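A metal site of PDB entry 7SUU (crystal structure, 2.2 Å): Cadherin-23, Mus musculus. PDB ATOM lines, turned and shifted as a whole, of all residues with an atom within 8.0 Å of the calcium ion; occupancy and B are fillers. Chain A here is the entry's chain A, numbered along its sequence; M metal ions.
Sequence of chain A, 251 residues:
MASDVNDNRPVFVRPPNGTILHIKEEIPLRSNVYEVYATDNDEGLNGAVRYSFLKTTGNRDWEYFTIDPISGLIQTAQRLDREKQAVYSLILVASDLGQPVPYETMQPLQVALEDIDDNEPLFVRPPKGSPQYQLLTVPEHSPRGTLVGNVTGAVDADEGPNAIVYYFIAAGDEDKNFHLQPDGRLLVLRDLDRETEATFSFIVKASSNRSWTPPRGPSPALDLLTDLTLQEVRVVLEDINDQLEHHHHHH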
ATOM      1  N   VAL A   5      14.536 -11.543   9.271  1.00  0.00           N
ATOM      2  CA  VAL A   5      14.915 -12.968   9.565  1.00  0.00           C
ATOM      3  C   VAL A   5      15.830 -12.978  10.803  1.00  0.00           C
ATOM      4  O   VAL A   5      16.586 -11.995  10.984  1.00  0.00           O
ATOM      5  CB  VAL A   5      15.595 -13.665   8.357  1.00  0.00           C
ATOM      6  CG1 VAL A   5      15.603 -15.182   8.507  1.00  0.00           C
ATOM      7  CG2 VAL A   5      14.940 -13.282   7.038  1.00  0.00           C
ATOM      8  N   ASN A   6      15.731 -14.035  11.623  1.00  0.00           N
ATOM      9  CA  ASN A   6      16.391 -14.154  12.953  1.00  0.00           C
ATOM     10  C   ASN A   6      17.713 -14.920  12.763  1.00  0.00           C
ATOM     11  O   ASN A   6      17.699 -16.164  12.899  1.00  0.00           O
ATOM     12  CB  ASN A   6      15.437 -14.782  13.979  1.00  0.00           C
ATOM     13  CG  ASN A   6      15.921 -14.697  15.417  1.00  0.00           C
ATOM     14  OD1 ASN A   6      16.823 -13.922  15.745  1.00  0.00           O
ATOM     15  ND2 ASN A   6      15.322 -15.483  16.293  1.00  0.00           N
ATOM     16  N   ASP A   7      18.799 -14.195  12.463  1.00  0.00           N
ATOM     17  CA  ASP A   7      20.092 -14.775  12.000  1.00  0.00           C
ATOM     18  C   ASP A   7      20.883 -15.336  13.186  1.00  0.00           C
ATOM     19  O   ASP A   7      21.408 -16.445  13.058  1.00  0.00           O
ATOM     20  CB  ASP A   7      20.937 -13.749  11.234  1.00  0.00           C
ATOM     21  CG  ASP A   7      20.285 -13.218   9.963  1.00  0.00           C
ATOM     22  OD1 ASP A   7      19.455 -13.938   9.368  1.00  0.00           O
ATOM     23  OD2 ASP A   7      20.615 -12.067   9.573  1.00  0.00           O
ATOM     24  N   ASN A   8      20.946 -14.575  14.286  1.00  0.00           N
ATOM     25  CA  ASN A   8      21.830 -14.791  15.468  1.00  0.00           C
ATOM     26  C   ASN A   8      21.035 -15.369  16.650  1.00  0.00           C
ATOM     27  O   ASN A   8      19.861 -15.006  16.857  1.00  0.00           O
ATOM     28  CB  ASN A   8      22.515 -13.487  15.917  1.00  0.00           C
ATOM     29  CG  ASN A   8      23.554 -13.012  14.928  1.00  0.00           C
ATOM     30  OD1 ASN A   8      24.266 -13.833  14.364  1.00  0.00           O
ATOM     31  ND2 ASN A   8      23.648 -11.714  14.696  1.00  0.00           N
ATOM     32  N   ARG A   9      21.697 -16.241  17.398  1.00  0.00           N
ATOM     33  CA  ARG A   9      21.276 -16.802  18.692  1.00  0.00           C
ATOM     34  C   ARG A   9      21.907 -15.934  19.784  1.00  0.00           C
ATOM     35  O   ARG A   9      22.992 -15.416  19.559  1.00  0.00           O
ATOM     36  CB  ARG A   9      21.789 -18.239  18.698  1.00  0.00           C
ATOM     37  CG  ARG A   9      20.969 -19.215  19.515  1.00  0.00           C
ATOM     38  CD  ARG A   9      21.854 -19.972  20.477  1.00  0.00           C
ATOM     39  NE  ARG A   9      22.744 -20.920  19.843  1.00  0.00           N
ATOM     40  CZ  ARG A   9      23.904 -21.329  20.364  1.00  0.00           C
ATOM     41  NH1 ARG A   9      24.353 -20.813  21.504  1.00  0.00           N
ATOM     42  NH2 ARG A   9      24.630 -22.210  19.703  1.00  0.00           N
ATOM     43  N   PRO A  10      21.281 -15.704  20.970  1.00  0.00           N
ATOM     44  CA  PRO A  10      21.956 -14.996  22.065  1.00  0.00           C
ATOM     45  C   PRO A  10      23.194 -15.730  22.575  1.00  0.00           C
ATOM     46  O   PRO A  10      23.239 -16.935  22.583  1.00  0.00           O
ATOM     47  CB  PRO A  10      20.919 -14.884  23.191  1.00  0.00           C
ATOM     48  CG  PRO A  10      19.604 -15.216  22.531  1.00  0.00           C
ATOM     49  CD  PRO A  10      19.922 -16.085  21.330  1.00  0.00           C
ATOM     50  N   THR A  39      24.072 -11.181  24.766  1.00  0.00           N
ATOM     51  CA  THR A  39      23.905 -10.220  23.638  1.00  0.00           C
ATOM     52  C   THR A  39      23.333 -10.960  22.431  1.00  0.00           C
ATOM     53  O   THR A  39      23.641 -12.164  22.252  1.00  0.00           O
ATOM     54  CB  THR A  39      25.259  -9.615  23.261  1.00  0.00           C
ATOM     55  OG1 THR A  39      26.103 -10.761  23.115  1.00  0.00           O
ATOM     56  CG2 THR A  39      25.818  -8.683  24.307  1.00  0.00           C
ATOM     57  N   ASP A  40      22.575 -10.267  21.606  1.00  0.00           N
ATOM     58  CA  ASP A  40      22.052 -10.764  20.316  1.00  0.00           C
ATOM     59  C   ASP A  40      22.128  -9.571  19.341  1.00  0.00           C
ATOM     60  O   ASP A  40      21.542  -8.514  19.653  1.00  0.00           O
ATOM     61  CB  ASP A  40      20.635 -11.293  20.500  1.00  0.00           C
ATOM     62  CG  ASP A  40      20.059 -12.161  19.387  1.00  0.00           C
ATOM     63  OD1 ASP A  40      20.310 -11.900  18.187  1.00  0.00           O
ATOM     64  OD2 ASP A  40      19.293 -13.063  19.728  1.00  0.00           O
ATOM     65  N   ASN A  41      22.819  -9.741  18.227  1.00  0.00           N
ATOM     66  CA  ASN A  41      23.185  -8.643  17.300  1.00  0.00           C
ATOM     67  C   ASN A  41      22.114  -8.522  16.198  1.00  0.00           C
ATOM     68  O   ASN A  41      22.394  -7.873  15.203  1.00  0.00           O
ATOM     69  CB  ASN A  41      24.577  -8.842  16.703  1.00  0.00           C
ATOM     70  CG  ASN A  41      25.552  -9.473  17.681  1.00  0.00           C
ATOM     71  OD1 ASN A  41      25.698  -9.018  18.821  1.00  0.00           O
ATOM     72  ND2 ASN A  41      26.205 -10.544  17.259  1.00  0.00           N
ATOM     73  N   ASP A  42      20.947  -9.135  16.364  1.00  0.00           N
ATOM     74  CA  ASP A  42      19.862  -9.061  15.353  1.00  0.00           C
ATOM     75  C   ASP A  42      19.060  -7.773  15.526  1.00  0.00           C
ATOM     76  O   ASP A  42      19.152  -7.166  16.610  1.00  0.00           O
ATOM     77  CB  ASP A  42      18.928 -10.268  15.427  1.00  0.00           C
ATOM     78  CG  ASP A  42      19.536 -11.507  14.791  1.00  0.00           C
ATOM     79  OD1 ASP A  42      20.280 -11.343  13.802  1.00  0.00           O
ATOM     80  OD2 ASP A  42      19.273 -12.622  15.312  1.00  0.00           O
ATOM     81  N   GLU A  43      18.309  -7.412  14.487  1.00  0.00           N
ATOM     82  CA  GLU A  43      17.491  -6.167  14.364  1.00  0.00           C
ATOM     83  C   GLU A  43      16.202  -6.315  15.181  1.00  0.00           C
ATOM     84  O   GLU A  43      15.491  -7.337  14.990  1.00  0.00           O
ATOM     85  CB  GLU A  43      17.201  -5.865  12.880  1.00  0.00           C
ATOM     86  CG  GLU A  43      16.222  -6.840  12.197  1.00  0.00           C
ATOM     87  CD  GLU A  43      16.234  -6.944  10.673  1.00  0.00           C
ATOM     88  OE1 GLU A  43      17.141  -6.353  10.029  1.00  0.00           O
ATOM     89  OE2 GLU A  43      15.342  -7.626  10.113  1.00  0.00           O
ATOM     90  N   GLY A  44      15.911  -5.330  16.042  1.00  0.00           N
ATOM     91  CA  GLY A  44      14.645  -5.229  16.802  1.00  0.00           C
ATOM     92  C   GLY A  44      14.411  -6.443  17.684  1.00  0.00           C
ATOM     93  O   GLY A  44      15.332  -6.781  18.471  1.00  0.00           O
ATOM     94  N   LEU A  45      13.258  -7.113  17.516  1.00  0.00           N
ATOM     95  CA  LEU A  45      12.751  -8.178  18.440  1.00  0.00           C
ATOM     96  C   LEU A  45      13.589  -9.463  18.331  1.00  0.00           C
ATOM     97  O   LEU A  45      13.930 -10.050  19.380  1.00  0.00           O
ATOM     98  CB  LEU A  45      11.257  -8.419  18.188  1.00  0.00           C
ATOM     99  CG  LEU A  45      10.359  -7.730  19.209  1.00  0.00           C
ATOM    100  CD1 LEU A  45      10.640  -6.232  19.252  1.00  0.00           C
ATOM    101  CD2 LEU A  45       8.891  -7.992  18.925  1.00  0.00           C
ATOM    102  N   ASN A  46      13.993  -9.846  17.121  1.00  0.00           N
ATOM    103  CA  ASN A  46      14.993 -10.912  16.871  1.00  0.00           C
ATOM    104  C   ASN A  46      16.263 -10.697  17.708  1.00  0.00           C
ATOM    105  O   ASN A  46      17.013 -11.679  17.849  1.00  0.00           O
ATOM    106  CB  ASN A  46      15.329 -10.979  15.382  1.00  0.00           C
ATOM    107  CG  ASN A  46      14.099 -11.242  14.540  1.00  0.00           C
ATOM    108  OD1 ASN A  46      13.163 -11.903  14.971  1.00  0.00           O
ATOM    109  ND2 ASN A  46      14.100 -10.687  13.344  1.00  0.00           N
ATOM    110  N   GLY A  47      16.535  -9.486  18.189  1.00  0.00           N
ATOM    111  CA  GLY A  47      17.730  -9.144  18.994  1.00  0.00           C
ATOM    112  C   GLY A  47      17.400  -8.607  20.380  1.00  0.00           C
ATOM    113  O   GLY A  47      18.345  -8.144  21.050  1.00  0.00           O
ATOM    114  N   ALA A  48      16.145  -8.674  20.830  1.00  0.00           N
ATOM    115  CA  ALA A  48      15.775  -8.354  22.232  1.00  0.00           C
ATOM    116  C   ALA A  48      16.061  -9.586  23.101  1.00  0.00           C
ATOM    117  O   ALA A  48      15.667 -10.674  22.681  1.00  0.00           O
ATOM    118  CB  ALA A  48      14.325  -7.957  22.332  1.00  0.00           C
ATOM    119  N   VAL A  49      16.761  -9.451  24.224  1.00  0.00           N
ATOM    120  CA  VAL A  49      17.099 -10.621  25.085  1.00  0.00           C
ATOM    121  C   VAL A  49      16.191 -10.632  26.321  1.00  0.00           C
ATOM    122  O   VAL A  49      16.036  -9.566  26.976  1.00  0.00           O
ATOM    123  CB  VAL A  49      18.587 -10.675  25.466  1.00  0.00           C
ATOM    124  CG1 VAL A  49      18.888 -11.843  26.398  1.00  0.00           C
ATOM    125  CG2 VAL A  49      19.477 -10.786  24.229  1.00  0.00           C
ATOM    126  N   SER A  95      16.785 -15.817  25.790  1.00  0.00           N
ATOM    127  CA  SER A  95      15.906 -15.944  24.600  1.00  0.00           C
ATOM    128  C   SER A  95      15.807 -14.584  23.924  1.00  0.00           C
ATOM    129  O   SER A  95      15.802 -13.578  24.625  1.00  0.00           O
ATOM    130  CB  SER A  95      14.503 -16.410  24.924  1.00  0.00           C
ATOM    131  OG  SER A  95      14.500 -17.237  26.061  1.00  0.00           O
ATOM    132  N   ASP A  96      15.762 -14.596  22.609  1.00  0.00           N
ATOM    133  CA  ASP A  96      15.288 -13.439  21.813  1.00  0.00           C
ATOM    134  C   ASP A  96      13.772 -13.603  21.678  1.00  0.00           C
ATOM    135  O   ASP A  96      13.195 -14.554  22.273  1.00  0.00           O
ATOM    136  CB  ASP A  96      16.050 -13.327  20.498  1.00  0.00           C
ATOM    137  CG  ASP A  96      15.804 -14.452  19.503  1.00  0.00           C
ATOM    138  OD1 ASP A  96      14.710 -15.048  19.554  1.00  0.00           O
ATOM    139  OD2 ASP A  96      16.692 -14.681  18.655  1.00  0.00           O
ATOM    140  N   LEU A  97      13.140 -12.639  21.023  1.00  0.00           N
ATOM    141  CA  LEU A  97      11.671 -12.641  20.779  1.00  0.00           C
ATOM    142  C   LEU A  97      11.425 -12.792  19.285  1.00  0.00           C
ATOM    143  O   LEU A  97      10.645 -12.021  18.764  1.00  0.00           O
ATOM    144  CB  LEU A  97      11.117 -11.345  21.382  1.00  0.00           C
ATOM    145  CG  LEU A  97      11.193 -11.300  22.914  1.00  0.00           C
ATOM    146  CD1 LEU A  97      10.833  -9.930  23.466  1.00  0.00           C
ATOM    147  CD2 LEU A  97      10.296 -12.388  23.501  1.00  0.00           C
ATOM    148  N   GLY A  98      12.043 -13.785  18.638  1.00  0.00           N
ATOM    149  CA  GLY A  98      11.846 -14.179  17.217  1.00  0.00           C
ATOM    150  C   GLY A  98      10.407 -14.508  16.818  1.00  0.00           C
ATOM    151  O   GLY A  98       9.583 -14.863  17.724  1.00  0.00           O
ATOM    152  N   GLN A  99      10.167 -14.469  15.490  1.00  0.00           N
ATOM    153  CA  GLN A  99       8.854 -14.372  14.759  1.00  0.00           C
ATOM    154  C   GLN A  99       7.800 -15.291  15.396  1.00  0.00           C
ATOM    155  O   GLN A  99       7.118 -14.796  16.292  1.00  0.00           O
ATOM    156  CB  GLN A  99       9.040 -14.623  13.265  1.00  0.00           C
ATOM    157  CG  GLN A  99       9.743 -13.489  12.529  1.00  0.00           C
ATOM    158  CD  GLN A  99      11.226 -13.775  12.498  1.00  0.00           C
ATOM    159  OE1 GLN A  99      11.764 -14.364  13.428  1.00  0.00           O
ATOM    160  NE2 GLN A  99      11.878 -13.365  11.413  1.00  0.00           N
ATOM    161  N   PRO A 102      11.362 -18.058  19.080  1.00  0.00           N
ATOM    162  CA  PRO A 102      12.661 -17.488  19.438  1.00  0.00           C
ATOM    163  C   PRO A 102      13.805 -18.511  19.491  1.00  0.00           C
ATOM    164  O   PRO A 102      13.525 -19.665  19.777  1.00  0.00           O
ATOM    165  CB  PRO A 102      12.372 -16.962  20.853  1.00  0.00           C
ATOM    166  CG  PRO A 102      11.367 -17.950  21.439  1.00  0.00           C
ATOM    167  CD  PRO A 102      10.509 -18.345  20.250  1.00  0.00           C
ATOM    168  N   TYR A 103      15.028 -18.092  19.174  1.00  0.00           N
ATOM    169  CA  TYR A 103      16.291 -18.810  19.499  1.00  0.00           C
ATOM    170  C   TYR A 103      16.620 -18.527  20.974  1.00  0.00           C
ATOM    171  O   TYR A 103      16.338 -17.413  21.450  1.00  0.00           O
ATOM    172  CB  TYR A 103      17.430 -18.413  18.556  1.00  0.00           C
ATOM    173  CG  TYR A 103      17.250 -18.805  17.111  1.00  0.00           C
ATOM    174  CD1 TYR A 103      16.208 -19.616  16.698  1.00  0.00           C
ATOM    175  CD2 TYR A 103      18.152 -18.376  16.138  1.00  0.00           C
ATOM    176  CE1 TYR A 103      16.040 -19.973  15.367  1.00  0.00           C
ATOM    177  CE2 TYR A 103      18.000 -18.727  14.808  1.00  0.00           C
ATOM    178  CZ  TYR A 103      16.940 -19.539  14.418  1.00  0.00           C
ATOM    179  OH  TYR A 103      16.775 -19.905  13.115  1.00  0.00           O
ATOM    180  N   GLU A 104      17.099 -19.541  21.683  1.00  0.00           N
ATOM    181  CA  GLU A 104      17.444 -19.496  23.123  1.00  0.00           C
ATOM    182  C   GLU A 104      18.771 -20.241  23.321  1.00  0.00           C
ATOM    183  O   GLU A 104      19.065 -21.163  22.570  1.00  0.00           O
ATOM    184  CB  GLU A 104      16.394 -20.147  24.019  1.00  0.00           C
ATOM    185  CG  GLU A 104      14.961 -19.990  23.523  1.00  0.00           C
ATOM    186  CD  GLU A 104      13.866 -20.302  24.541  1.00  0.00           C
ATOM    187  OE1 GLU A 104      14.194 -20.574  25.702  1.00  0.00           O
ATOM    188  OE2 GLU A 104      12.678 -20.249  24.163  1.00  0.00           O
HETATM  189 CA    CA M   1      18.368 -13.322  17.499  1.00  0.00          CA
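O of Asn 46 is bound to the calcium ion (2.2 Å).
The calcium ion is bound by O of Asn 8 (2.3 Å).
The calcium ion is bound by the side-chain amide oxygen (OD1) of Asn 6 (2.4 Å).
The side-chain carboxylate (OD2) of Asp 40 binds the calcium ion (2.4 Å).
OD2 of Asp 96 is bound to the calcium ion.
The side-chain carboxylate (OD2) of Asp 42 is bound to the calcium ion (2.5 Å).
OD1 of Asp 40 binds the calcium ion, at 2.5 Å.
The side-chain carboxylate (OD1) of Asp 42 is in hydrogen-bond range of the backbone NH (N) of Asp 7, 3.5 Å away.
N of Tyr 103 sits at hydrogen-bond distance from OD1 of Asp 96 (3.1 Å).
The backbone NH (N) of Gly 98 sits at hydrogen-bond distance from the side-chain carboxylate (OD1) of Asp 96.
The side-chain amide oxygen of Gln 99 sits close to the side-chain amide oxygen of Asn 46, 3.2 Å away.
Of the 25 residues printed, 6 come within 4 Å of the calcium ion.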
